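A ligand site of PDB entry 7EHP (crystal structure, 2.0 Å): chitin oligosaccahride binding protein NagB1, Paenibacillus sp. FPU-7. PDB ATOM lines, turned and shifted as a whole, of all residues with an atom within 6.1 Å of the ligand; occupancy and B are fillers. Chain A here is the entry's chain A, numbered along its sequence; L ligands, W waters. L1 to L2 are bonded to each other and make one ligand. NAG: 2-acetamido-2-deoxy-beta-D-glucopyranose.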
ATOM      1  N   THR A   8      -0.435   2.495  -1.360  1.00  0.00           N
ATOM      2  CA  THR A   8       0.743   2.054  -0.628  1.00  0.00           C
ATOM      3  C   THR A   8       2.033   2.317  -1.382  1.00  0.00           C
ATOM      4  O   THR A   8       3.081   1.742  -1.027  1.00  0.00           O
ATOM      5  CB  THR A   8       0.633   0.554  -0.297  1.00  0.00           C
ATOM      6  OG1 THR A   8       0.597  -0.198  -1.507  1.00  0.00           O
ATOM      7  CG2 THR A   8      -0.636   0.281   0.491  1.00  0.00           C
ATOM      8  N   GLN A   9       2.013   3.166  -2.409  1.00  0.00           N
ATOM      9  CA  GLN A   9       3.195   3.391  -3.248  1.00  0.00           C
ATOM     10  C   GLN A   9       4.063   4.482  -2.612  1.00  0.00           C
ATOM     11  O   GLN A   9       4.129   5.615  -3.085  1.00  0.00           O
ATOM     12  CB  GLN A   9       2.787   3.728  -4.675  1.00  0.00           C
ATOM     13  CG  GLN A   9       1.886   2.700  -5.385  1.00  0.00           C
ATOM     14  CD  GLN A   9       2.345   1.260  -5.144  1.00  0.00           C
ATOM     15  OE1 GLN A   9       3.508   0.910  -5.383  1.00  0.00           O
ATOM     16  NE2 GLN A   9       1.425   0.414  -4.684  1.00  0.00           N
ATOM     17  N   ARG A  17       5.284   4.421 -10.077  1.00  0.00           N
ATOM     18  CA  ARG A  17       3.923   3.970  -9.761  1.00  0.00           C
ATOM     19  C   ARG A  17       3.118   5.083  -9.084  1.00  0.00           C
ATOM     20  O   ARG A  17       1.919   5.216  -9.345  1.00  0.00           O
ATOM     21  CB  ARG A  17       3.959   2.732  -8.878  1.00  0.00           C
ATOM     22  CG  ARG A  17       4.638   1.528  -9.527  1.00  0.00           C
ATOM     23  CD  ARG A  17       4.387   0.253  -8.739  1.00  0.00           C
ATOM     24  NE  ARG A  17       3.087  -0.325  -9.049  1.00  0.00           N
ATOM     25  CZ  ARG A  17       2.677  -1.513  -8.601  1.00  0.00           C
ATOM     26  NH1 ARG A  17       3.467  -2.225  -7.811  1.00  0.00           N
ATOM     27  NH2 ARG A  17       1.466  -1.978  -8.914  1.00  0.00           N
ATOM     28  N   ASP A  44       2.589  -0.447   3.018  1.00  0.00           N
ATOM     29  CA  ASP A  44       1.781  -1.626   2.723  1.00  0.00           C
ATOM     30  C   ASP A  44       1.269  -2.363   3.970  1.00  0.00           C
ATOM     31  O   ASP A  44       0.063  -2.505   4.155  1.00  0.00           O
ATOM     32  CB  ASP A  44       2.572  -2.587   1.813  1.00  0.00           C
ATOM     33  CG  ASP A  44       3.964  -2.973   2.370  1.00  0.00           C
ATOM     34  OD1 ASP A  44       4.294  -2.734   3.556  1.00  0.00           O
ATOM     35  OD2 ASP A  44       4.743  -3.537   1.572  1.00  0.00           O
ATOM     36  N   LYS A  45       2.185  -2.877   4.804  1.00  0.00           N
ATOM     37  CA  LYS A  45       1.764  -3.651   5.963  1.00  0.00           C
ATOM     38  C   LYS A  45       1.017  -2.787   6.974  1.00  0.00           C
ATOM     39  O   LYS A  45       0.139  -3.283   7.677  1.00  0.00           O
ATOM     40  CB  LYS A  45       2.979  -4.293   6.628  1.00  0.00           C
ATOM     41  CG  LYS A  45       3.956  -3.301   7.277  1.00  0.00           C
ATOM     42  CD  LYS A  45       5.147  -4.019   7.914  1.00  0.00           C
ATOM     43  CE  LYS A  45       5.871  -3.097   8.876  1.00  0.00           C
ATOM     44  NZ  LYS A  45       6.983  -3.762   9.609  1.00  0.00           N
ATOM     45  N   ARG A  48      -2.577  -2.346   5.332  1.00  0.00           N
ATOM     46  CA  ARG A  48      -3.395  -3.550   5.180  1.00  0.00           C
ATOM     47  C   ARG A  48      -3.734  -4.170   6.529  1.00  0.00           C
ATOM     48  O   ARG A  48      -4.864  -4.623   6.745  1.00  0.00           O
ATOM     49  CB  ARG A  48      -2.682  -4.565   4.293  1.00  0.00           C
ATOM     50  CG  ARG A  48      -3.567  -5.763   3.976  1.00  0.00           C
ATOM     51  CD  ARG A  48      -2.819  -6.839   3.245  1.00  0.00           C
ATOM     52  NE  ARG A  48      -3.682  -7.982   2.955  1.00  0.00           N
ATOM     53  CZ  ARG A  48      -3.238  -9.135   2.462  1.00  0.00           C
ATOM     54  NH1 ARG A  48      -1.939  -9.302   2.215  1.00  0.00           N
ATOM     55  NH2 ARG A  48      -4.101 -10.114   2.201  1.00  0.00           N
ATOM     56  N   PHE A  49      -2.778  -4.200   7.449  1.00  0.00           N
ATOM     57  CA  PHE A  49      -2.905  -4.984   8.660  1.00  0.00           C
ATOM     58  C   PHE A  49      -3.269  -4.170   9.898  1.00  0.00           C
ATOM     59  O   PHE A  49      -3.589  -4.770  10.926  1.00  0.00           O
ATOM     60  CB  PHE A  49      -1.605  -5.775   8.931  1.00  0.00           C
ATOM     61  CG  PHE A  49      -1.195  -6.664   7.796  1.00  0.00           C
ATOM     62  CD1 PHE A  49      -2.138  -7.416   7.107  1.00  0.00           C
ATOM     63  CD2 PHE A  49       0.127  -6.758   7.415  1.00  0.00           C
ATOM     64  CE1 PHE A  49      -1.769  -8.238   6.078  1.00  0.00           C
ATOM     65  CE2 PHE A  49       0.506  -7.568   6.381  1.00  0.00           C
ATOM     66  CZ  PHE A  49      -0.445  -8.311   5.699  1.00  0.00           C
ATOM     67  N   ASP A  66      -6.311   1.060  -1.422  1.00  0.00           N
ATOM     68  CA  ASP A  66      -5.612  -0.186  -1.693  1.00  0.00           C
ATOM     69  C   ASP A  66      -6.247  -1.309  -0.887  1.00  0.00           C
ATOM     70  O   ASP A  66      -6.312  -1.249   0.344  1.00  0.00           O
ATOM     71  CB  ASP A  66      -4.130  -0.009  -1.340  1.00  0.00           C
ATOM     72  CG  ASP A  66      -3.287  -1.177  -1.768  1.00  0.00           C
ATOM     73  OD1 ASP A  66      -3.547  -2.305  -1.325  1.00  0.00           O
ATOM     74  OD2 ASP A  66      -2.365  -0.950  -2.583  1.00  0.00           O
ATOM     75  N   PHE A  68      -7.073  -5.783  -0.590  1.00  0.00           N
ATOM     76  CA  PHE A  68      -6.743  -7.157  -0.960  1.00  0.00           C
ATOM     77  C   PHE A  68      -7.998  -8.015  -1.036  1.00  0.00           C
ATOM     78  O   PHE A  68      -8.916  -7.878  -0.217  1.00  0.00           O
ATOM     79  CB  PHE A  68      -5.737  -7.799   0.024  1.00  0.00           C
ATOM     80  CG  PHE A  68      -4.327  -7.450  -0.302  1.00  0.00           C
ATOM     81  CD1 PHE A  68      -3.821  -6.196   0.032  1.00  0.00           C
ATOM     82  CD2 PHE A  68      -3.522  -8.322  -1.005  1.00  0.00           C
ATOM     83  CE1 PHE A  68      -2.517  -5.839  -0.285  1.00  0.00           C
ATOM     84  CE2 PHE A  68      -2.214  -7.965  -1.331  1.00  0.00           C
ATOM     85  CZ  PHE A  68      -1.718  -6.711  -0.980  1.00  0.00           C
ATOM     86  N   THR A 115      -5.497  -4.496  -9.771  1.00  0.00           N
ATOM     87  CA  THR A 115      -4.752  -3.699 -10.721  1.00  0.00           C
ATOM     88  C   THR A 115      -3.599  -4.462 -11.338  1.00  0.00           C
ATOM     89  O   THR A 115      -2.996  -3.968 -12.289  1.00  0.00           O
ATOM     90  CB  THR A 115      -4.165  -2.436 -10.089  1.00  0.00           C
ATOM     91  OG1 THR A 115      -3.365  -2.794  -8.958  1.00  0.00           O
ATOM     92  CG2 THR A 115      -5.279  -1.427  -9.694  1.00  0.00           C
ATOM     93  N   ALA A 116      -3.264  -5.630 -10.789  1.00  0.00           N
ATOM     94  CA  ALA A 116      -2.118  -6.392 -11.248  1.00  0.00           C
ATOM     95  C   ALA A 116      -2.405  -7.878 -11.133  1.00  0.00           C
ATOM     96  O   ALA A 116      -3.202  -8.318 -10.313  1.00  0.00           O
ATOM     97  CB  ALA A 116      -0.860  -6.062 -10.453  1.00  0.00           C
ATOM     98  N   PHE A 118       0.033 -11.062 -10.121  1.00  0.00           N
ATOM     99  CA  PHE A 118       1.331 -11.288  -9.497  1.00  0.00           C
ATOM    100  C   PHE A 118       1.705 -12.749  -9.626  1.00  0.00           C
ATOM    101  O   PHE A 118       0.828 -13.620  -9.707  1.00  0.00           O
ATOM    102  CB  PHE A 118       1.321 -10.849  -8.002  1.00  0.00           C
ATOM    103  CG  PHE A 118       0.798 -11.900  -7.038  1.00  0.00           C
ATOM    104  CD1 PHE A 118       1.646 -12.878  -6.512  1.00  0.00           C
ATOM    105  CD2 PHE A 118      -0.533 -11.904  -6.654  1.00  0.00           C
ATOM    106  CE1 PHE A 118       1.159 -13.844  -5.628  1.00  0.00           C
ATOM    107  CE2 PHE A 118      -1.027 -12.864  -5.785  1.00  0.00           C
ATOM    108  CZ  PHE A 118      -0.182 -13.833  -5.261  1.00  0.00           C
ATOM    109  N   GLU A 120       4.960 -15.079  -7.464  1.00  0.00           N
ATOM    110  CA  GLU A 120       6.105 -15.068  -6.560  1.00  0.00           C
ATOM    111  C   GLU A 120       7.020 -16.215  -6.935  1.00  0.00           C
ATOM    112  O   GLU A 120       6.543 -17.334  -7.143  1.00  0.00           O
ATOM    113  CB  GLU A 120       5.673 -15.204  -5.108  1.00  0.00           C
ATOM    114  CG  GLU A 120       5.013 -13.976  -4.551  1.00  0.00           C
ATOM    115  CD  GLU A 120       4.655 -14.137  -3.081  1.00  0.00           C
ATOM    116  OE1 GLU A 120       5.244 -15.007  -2.399  1.00  0.00           O
ATOM    117  OE2 GLU A 120       3.761 -13.376  -2.628  1.00  0.00           O
ATOM    118  N   TRP A 166       5.654 -10.233   6.936  1.00  0.00           N
ATOM    119  CA  TRP A 166       5.015 -10.859   5.780  1.00  0.00           C
ATOM    120  C   TRP A 166       6.045 -11.331   4.759  1.00  0.00           C
ATOM    121  O   TRP A 166       5.775 -12.263   3.997  1.00  0.00           O
ATOM    122  CB  TRP A 166       4.004  -9.889   5.139  1.00  0.00           C
ATOM    123  CG  TRP A 166       4.661  -8.757   4.414  1.00  0.00           C
ATOM    124  CD1 TRP A 166       5.040  -7.526   4.940  1.00  0.00           C
ATOM    125  CD2 TRP A 166       5.047  -8.732   3.036  1.00  0.00           C
ATOM    126  NE1 TRP A 166       5.633  -6.764   3.959  1.00  0.00           N
ATOM    127  CE2 TRP A 166       5.646  -7.482   2.789  1.00  0.00           C
ATOM    128  CE3 TRP A 166       4.924  -9.648   1.989  1.00  0.00           C
ATOM    129  CZ2 TRP A 166       6.123  -7.122   1.520  1.00  0.00           C
ATOM    130  CZ3 TRP A 166       5.395  -9.288   0.728  1.00  0.00           C
ATOM    131  CH2 TRP A 166       5.996  -8.045   0.505  1.00  0.00           C
ATOM    132  N   MET A 170       6.656 -15.416   2.286  1.00  0.00           N
ATOM    133  CA  MET A 170       6.551 -15.566   0.841  1.00  0.00           C
ATOM    134  C   MET A 170       7.136 -16.922   0.444  1.00  0.00           C
ATOM    135  O   MET A 170       6.404 -17.821   0.006  1.00  0.00           O
ATOM    136  CB  MET A 170       7.266 -14.399   0.139  1.00  0.00           C
ATOM    137  CG  MET A 170       6.301 -13.230  -0.135  1.00  0.00           C
ATOM    138  SD  MET A 170       6.972 -11.934  -1.213  1.00  0.00           S
ATOM    139  CE  MET A 170       8.456 -11.371  -0.362  1.00  0.00           C
ATOM    140  N   TYR A 225      11.989  -4.841   4.345  1.00  0.00           N
ATOM    141  CA  TYR A 225      11.752  -5.479   3.060  1.00  0.00           C
ATOM    142  C   TYR A 225      12.675  -5.001   1.933  1.00  0.00           C
ATOM    143  O   TYR A 225      13.298  -5.814   1.244  1.00  0.00           O
ATOM    144  CB  TYR A 225      10.289  -5.263   2.664  1.00  0.00           C
ATOM    145  CG  TYR A 225       9.886  -5.809   1.299  1.00  0.00           C
ATOM    146  CD1 TYR A 225      10.325  -7.051   0.858  1.00  0.00           C
ATOM    147  CD2 TYR A 225       9.034  -5.081   0.475  1.00  0.00           C
ATOM    148  CE1 TYR A 225       9.931  -7.567  -0.397  1.00  0.00           C
ATOM    149  CE2 TYR A 225       8.634  -5.565  -0.771  1.00  0.00           C
ATOM    150  CZ  TYR A 225       9.073  -6.795  -1.200  1.00  0.00           C
ATOM    151  OH  TYR A 225       8.660  -7.270  -2.429  1.00  0.00           O
ATOM    152  N   TRP A 245       5.959  -7.791  -8.478  1.00  0.00           N
ATOM    153  CA  TRP A 245       5.905  -6.337  -8.260  1.00  0.00           C
ATOM    154  C   TRP A 245       7.282  -5.768  -7.906  1.00  0.00           C
ATOM    155  O   TRP A 245       7.476  -4.552  -7.981  1.00  0.00           O
ATOM    156  CB  TRP A 245       4.913  -5.997  -7.142  1.00  0.00           C
ATOM    157  CG  TRP A 245       5.314  -6.621  -5.833  1.00  0.00           C
ATOM    158  CD1 TRP A 245       6.271  -6.166  -4.951  1.00  0.00           C
ATOM    159  CD2 TRP A 245       4.814  -7.846  -5.288  1.00  0.00           C
ATOM    160  NE1 TRP A 245       6.380  -7.043  -3.887  1.00  0.00           N
ATOM    161  CE2 TRP A 245       5.494  -8.071  -4.071  1.00  0.00           C
ATOM    162  CE3 TRP A 245       3.864  -8.773  -5.712  1.00  0.00           C
ATOM    163  CZ2 TRP A 245       5.236  -9.188  -3.281  1.00  0.00           C
ATOM    164  CZ3 TRP A 245       3.608  -9.880  -4.932  1.00  0.00           C
ATOM    165  CH2 TRP A 245       4.292 -10.073  -3.723  1.00  0.00           C
ATOM    166  N   ASN A 279       3.021 -19.739  -7.068  1.00  0.00           N
ATOM    167  CA  ASN A 279       2.215 -18.786  -6.317  1.00  0.00           C
ATOM    168  C   ASN A 279       1.881 -17.585  -7.209  1.00  0.00           C
ATOM    169  O   ASN A 279       2.781 -16.901  -7.708  1.00  0.00           O
ATOM    170  CB  ASN A 279       2.977 -18.369  -5.052  1.00  0.00           C
ATOM    171  CG  ASN A 279       2.200 -17.416  -4.158  1.00  0.00           C
ATOM    172  OD1 ASN A 279       2.792 -16.671  -3.369  1.00  0.00           O
ATOM    173  ND2 ASN A 279       0.871 -17.448  -4.245  1.00  0.00           N
ATOM    174  N   SER A 283      -4.772 -10.408  -6.817  1.00  0.00           N
ATOM    175  CA  SER A 283      -5.082 -10.273  -5.390  1.00  0.00           C
ATOM    176  C   SER A 283      -5.265  -8.843  -4.911  1.00  0.00           C
ATOM    177  O   SER A 283      -5.935  -8.635  -3.892  1.00  0.00           O
ATOM    178  CB  SER A 283      -3.944 -10.885  -4.571  1.00  0.00           C
ATOM    179  OG  SER A 283      -2.768 -10.158  -4.832  1.00  0.00           O
ATOM    180  N   ASN A 284      -4.633  -7.868  -5.563  1.00  0.00           N
ATOM    181  CA  ASN A 284      -4.443  -6.544  -4.992  1.00  0.00           C
ATOM    182  C   ASN A 284      -4.802  -5.467  -6.007  1.00  0.00           C
ATOM    183  O   ASN A 284      -4.305  -5.485  -7.141  1.00  0.00           O
ATOM    184  CB  ASN A 284      -2.992  -6.328  -4.529  1.00  0.00           C
ATOM    185  CG  ASN A 284      -2.814  -5.014  -3.782  1.00  0.00           C
ATOM    186  OD1 ASN A 284      -1.769  -4.368  -3.867  1.00  0.00           O
ATOM    187  ND2 ASN A 284      -3.849  -4.608  -3.042  1.00  0.00           N
ATOM    188  N   GLY A 285      -5.646  -4.545  -5.589  1.00  0.00           N
ATOM    189  CA  GLY A 285      -6.080  -3.444  -6.427  1.00  0.00           C
ATOM    190  C   GLY A 285      -6.701  -2.380  -5.567  1.00  0.00           C
ATOM    191  O   GLY A 285      -6.092  -1.982  -4.574  1.00  0.00           O
ATOM    192  N   ILE A 322       5.042  -4.386 -13.888  1.00  0.00           N
ATOM    193  CA  ILE A 322       3.867  -4.947 -13.240  1.00  0.00           C
ATOM    194  C   ILE A 322       2.987  -5.654 -14.261  1.00  0.00           C
ATOM    195  O   ILE A 322       2.529  -5.052 -15.246  1.00  0.00           O
ATOM    196  CB  ILE A 322       3.101  -3.879 -12.451  1.00  0.00           C
ATOM    197  CG1 ILE A 322       3.926  -3.458 -11.231  1.00  0.00           C
ATOM    198  CG2 ILE A 322       1.769  -4.403 -11.983  1.00  0.00           C
ATOM    199  CD1 ILE A 322       4.828  -2.392 -11.462  1.00  0.00           C
ATOM    200  N   ALA A 352      -1.953 -16.479  -2.729  1.00  0.00           N
ATOM    201  CA  ALA A 352      -1.206 -16.306  -1.493  1.00  0.00           C
ATOM    202  C   ALA A 352      -2.054 -16.784  -0.324  1.00  0.00           C
ATOM    203  O   ALA A 352      -3.277 -16.595  -0.309  1.00  0.00           O
ATOM    204  CB  ALA A 352      -0.831 -14.830  -1.307  1.00  0.00           C
ATOM    205  N   PHE A 353      -1.408 -17.385   0.676  1.00  0.00           N
ATOM    206  CA  PHE A 353      -2.132 -17.908   1.833  1.00  0.00           C
ATOM    207  C   PHE A 353      -2.949 -16.835   2.559  1.00  0.00           C
ATOM    208  O   PHE A 353      -4.010 -17.137   3.119  1.00  0.00           O
ATOM    209  CB  PHE A 353      -1.149 -18.580   2.814  1.00  0.00           C
ATOM    210  CG  PHE A 353      -0.452 -17.616   3.751  1.00  0.00           C
ATOM    211  CD1 PHE A 353       0.663 -16.903   3.329  1.00  0.00           C
ATOM    212  CD2 PHE A 353      -0.907 -17.444   5.041  1.00  0.00           C
ATOM    213  CE1 PHE A 353       1.296 -15.995   4.182  1.00  0.00           C
ATOM    214  CE2 PHE A 353      -0.275 -16.546   5.904  1.00  0.00           C
ATOM    215  CZ  PHE A 353       0.820 -15.829   5.471  1.00  0.00           C
ATOM    216  N   ASP A 354      -2.481 -15.587   2.583  1.00  0.00           N
ATOM    217  CA  ASP A 354      -3.224 -14.536   3.282  1.00  0.00           C
ATOM    218  C   ASP A 354      -4.520 -14.141   2.573  1.00  0.00           C
ATOM    219  O   ASP A 354      -5.311 -13.361   3.131  1.00  0.00           O
ATOM    220  CB  ASP A 354      -2.346 -13.301   3.435  1.00  0.00           C
ATOM    221  CG  ASP A 354      -1.763 -12.860   2.114  1.00  0.00           C
ATOM    222  OD1 ASP A 354      -2.399 -12.017   1.428  1.00  0.00           O
ATOM    223  OD2 ASP A 354      -0.706 -13.372   1.752  1.00  0.00           O
ATOM    224  N   ARG A 362      -2.654 -15.217   9.907  1.00  0.00           N
ATOM    225  CA  ARG A 362      -1.561 -14.564   9.205  1.00  0.00           C
ATOM    226  C   ARG A 362      -0.622 -13.844  10.179  1.00  0.00           C
ATOM    227  O   ARG A 362       0.600 -13.962  10.073  1.00  0.00           O
ATOM    228  CB  ARG A 362      -2.123 -13.555   8.187  1.00  0.00           C
ATOM    229  CG  ARG A 362      -1.101 -13.036   7.176  1.00  0.00           C
ATOM    230  CD  ARG A 362      -1.223 -11.532   6.967  1.00  0.00           C
ATOM    231  NE  ARG A 362      -0.636 -10.762   8.065  1.00  0.00           N
ATOM    232  CZ  ARG A 362      -1.341 -10.063   8.956  1.00  0.00           C
ATOM    233  NH1 ARG A 362      -2.661 -10.025   8.888  1.00  0.00           N
ATOM    234  NH2 ARG A 362      -0.709  -9.397   9.903  1.00  0.00           N
HETATM  235  C1  NAG L   1       2.347  -4.030  -4.131  1.00  0.00           C
HETATM  236  C2  NAG L   1       1.590  -5.232  -4.685  1.00  0.00           C
HETATM  237  C3  NAG L   1       1.196  -6.169  -3.540  1.00  0.00           C
HETATM  238  C4  NAG L   1       2.370  -6.452  -2.597  1.00  0.00           C
HETATM  239  C5  NAG L   1       3.134  -5.165  -2.265  1.00  0.00           C
HETATM  240  C6  NAG L   1       4.389  -5.354  -1.446  1.00  0.00           C
HETATM  241  C7  NAG L   1       0.446  -4.503  -6.744  1.00  0.00           C
HETATM  242  C8  NAG L   1      -0.875  -4.154  -7.354  1.00  0.00           C
HETATM  243  N2  NAG L   1       0.418  -4.834  -5.439  1.00  0.00           N
HETATM  244  O1  NAG L   1       2.671  -3.164  -5.169  1.00  0.00           O
HETATM  245  O3  NAG L   1       0.662  -7.371  -4.095  1.00  0.00           O
HETATM  246  O4  NAG L   1       1.815  -6.885  -1.352  1.00  0.00           O
HETATM  247  O5  NAG L   1       3.511  -4.465  -3.463  1.00  0.00           O
HETATM  248  O6  NAG L   1       4.842  -4.101  -0.935  1.00  0.00           O
HETATM  249  O7  NAG L   1       1.494  -4.472  -7.380  1.00  0.00           O
HETATM  250  C1  NAG L   2       1.875  -8.290  -1.128  1.00  0.00           C
HETATM  251  C2  NAG L   2       1.319  -8.529   0.273  1.00  0.00           C
HETATM  252  C3  NAG L   2       1.322 -10.014   0.588  1.00  0.00           C
HETATM  253  C4  NAG L   2       0.573 -10.781  -0.487  1.00  0.00           C
HETATM  254  C5  NAG L   2       1.142 -10.461  -1.866  1.00  0.00           C
HETATM  255  C6  NAG L   2       0.380 -11.114  -3.001  1.00  0.00           C
HETATM  256  C7  NAG L   2       1.419  -6.893   2.104  1.00  0.00           C
HETATM  257  C8  NAG L   2       2.291  -6.215   3.096  1.00  0.00           C
HETATM  258  N2  NAG L   2       2.033  -7.762   1.282  1.00  0.00           N
HETATM  259  O3  NAG L   2       0.713 -10.218   1.845  1.00  0.00           O
HETATM  260  O4  NAG L   2       0.667 -12.176  -0.267  1.00  0.00           O
HETATM  261  O5  NAG L   2       1.122  -9.043  -2.101  1.00  0.00           O
HETATM  262  O6  NAG L   2      -1.012 -10.825  -2.940  1.00  0.00           O
HETATM  263  O7  NAG L   2       0.208  -6.690   2.046  1.00  0.00           O
HETATM  264  O   HOH W   1       6.295  -2.853  -3.619  1.00  0.00           O
HETATM  265  O   HOH W   2       2.047  -6.940  -8.561  1.00  0.00           O
HETATM  266  O   HOH W   3       1.377 -12.326   3.466  1.00  0.00           O
HETATM  267  O   HOH W   4      -0.325  -3.762   1.104  1.00  0.00           O
HETATM  268  O   HOH W   5       0.015  -7.787  -6.996  1.00  0.00           O
HETATM  269  O   HOH W   6      -2.813 -12.098  -1.398  1.00  0.00           O
HETATM  270  O   HOH W   7       3.320  -1.485  -1.540  1.00  0.00           O
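OD2 of Asp 44 sits at hydrogen-bond distance from O6 of NAG L1, 2.6 Å away.
The side-chain hydroxyl of Ser 283 is in hydrogen-bond range of an oxygen (O6) of NAG L2 (2.7 Å).
An oxygen (O4) of NAG L2 sits at hydrogen-bond distance from the side-chain carboxylate (OD2) of Asp 354.
OD1 of Asn 284 is in hydrogen-bond range of N2 of NAG L1, at 2.7 Å.
NH1 of Arg 48 sits at hydrogen-bond distance from O3 of NAG L2 (2.8 Å).
NH1 of Arg 17 lies within hydrogen-bond range of O1 of NAG L1 (2.9 Å).
NH2 of Arg 48 is in salt-bridge range of OD1 of Asp 354, 2.7 Å away.
N of Thr 115 is in hydrogen-bond range of O of Asn 284, 3.1 Å away.
OD1 of Asp 66 sits at hydrogen-bond distance from ND2 of Asn 284 (2.9 Å).
The backbone NH of Ala 352 sits close to the side-chain amide nitrogen of Asn 279.
The indole nitrogen (NE1) of Trp 245 sits at hydrogen-bond distance from the side-chain hydroxyl (OH) of Tyr 225, 2.7 Å away.
The side-chain amide nitrogen of Gln 9 lies within hydrogen-bond range of the side-chain hydroxyl of Thr 8.
The backbone NH of Glu 120 is in hydrogen-bond range of the backbone carbonyl oxygen of Asn 279 (2.9 Å).
Water W6 lies within hydrogen-bond range of O6 of NAG L2 and OD1 of Asp 354.
Water W3 bridges an oxygen (O3) of NAG L2 (2.7 Å) and the side-chain carboxylate of Asp 354 (2.9 Å).
Water W7 lies within hydrogen-bond range of OG1 of Thr 8 and O6 of NAG L1.
Water W4 bridges O7 of NAG L2 and O of Asp 44.
Residues that only touch the ligand: Ala 352, Thr 115, Phe 68, Trp 166, Phe 118, Trp 245, Ala 116, Lys 45, Gln 9, Phe 49 and Glu 120.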
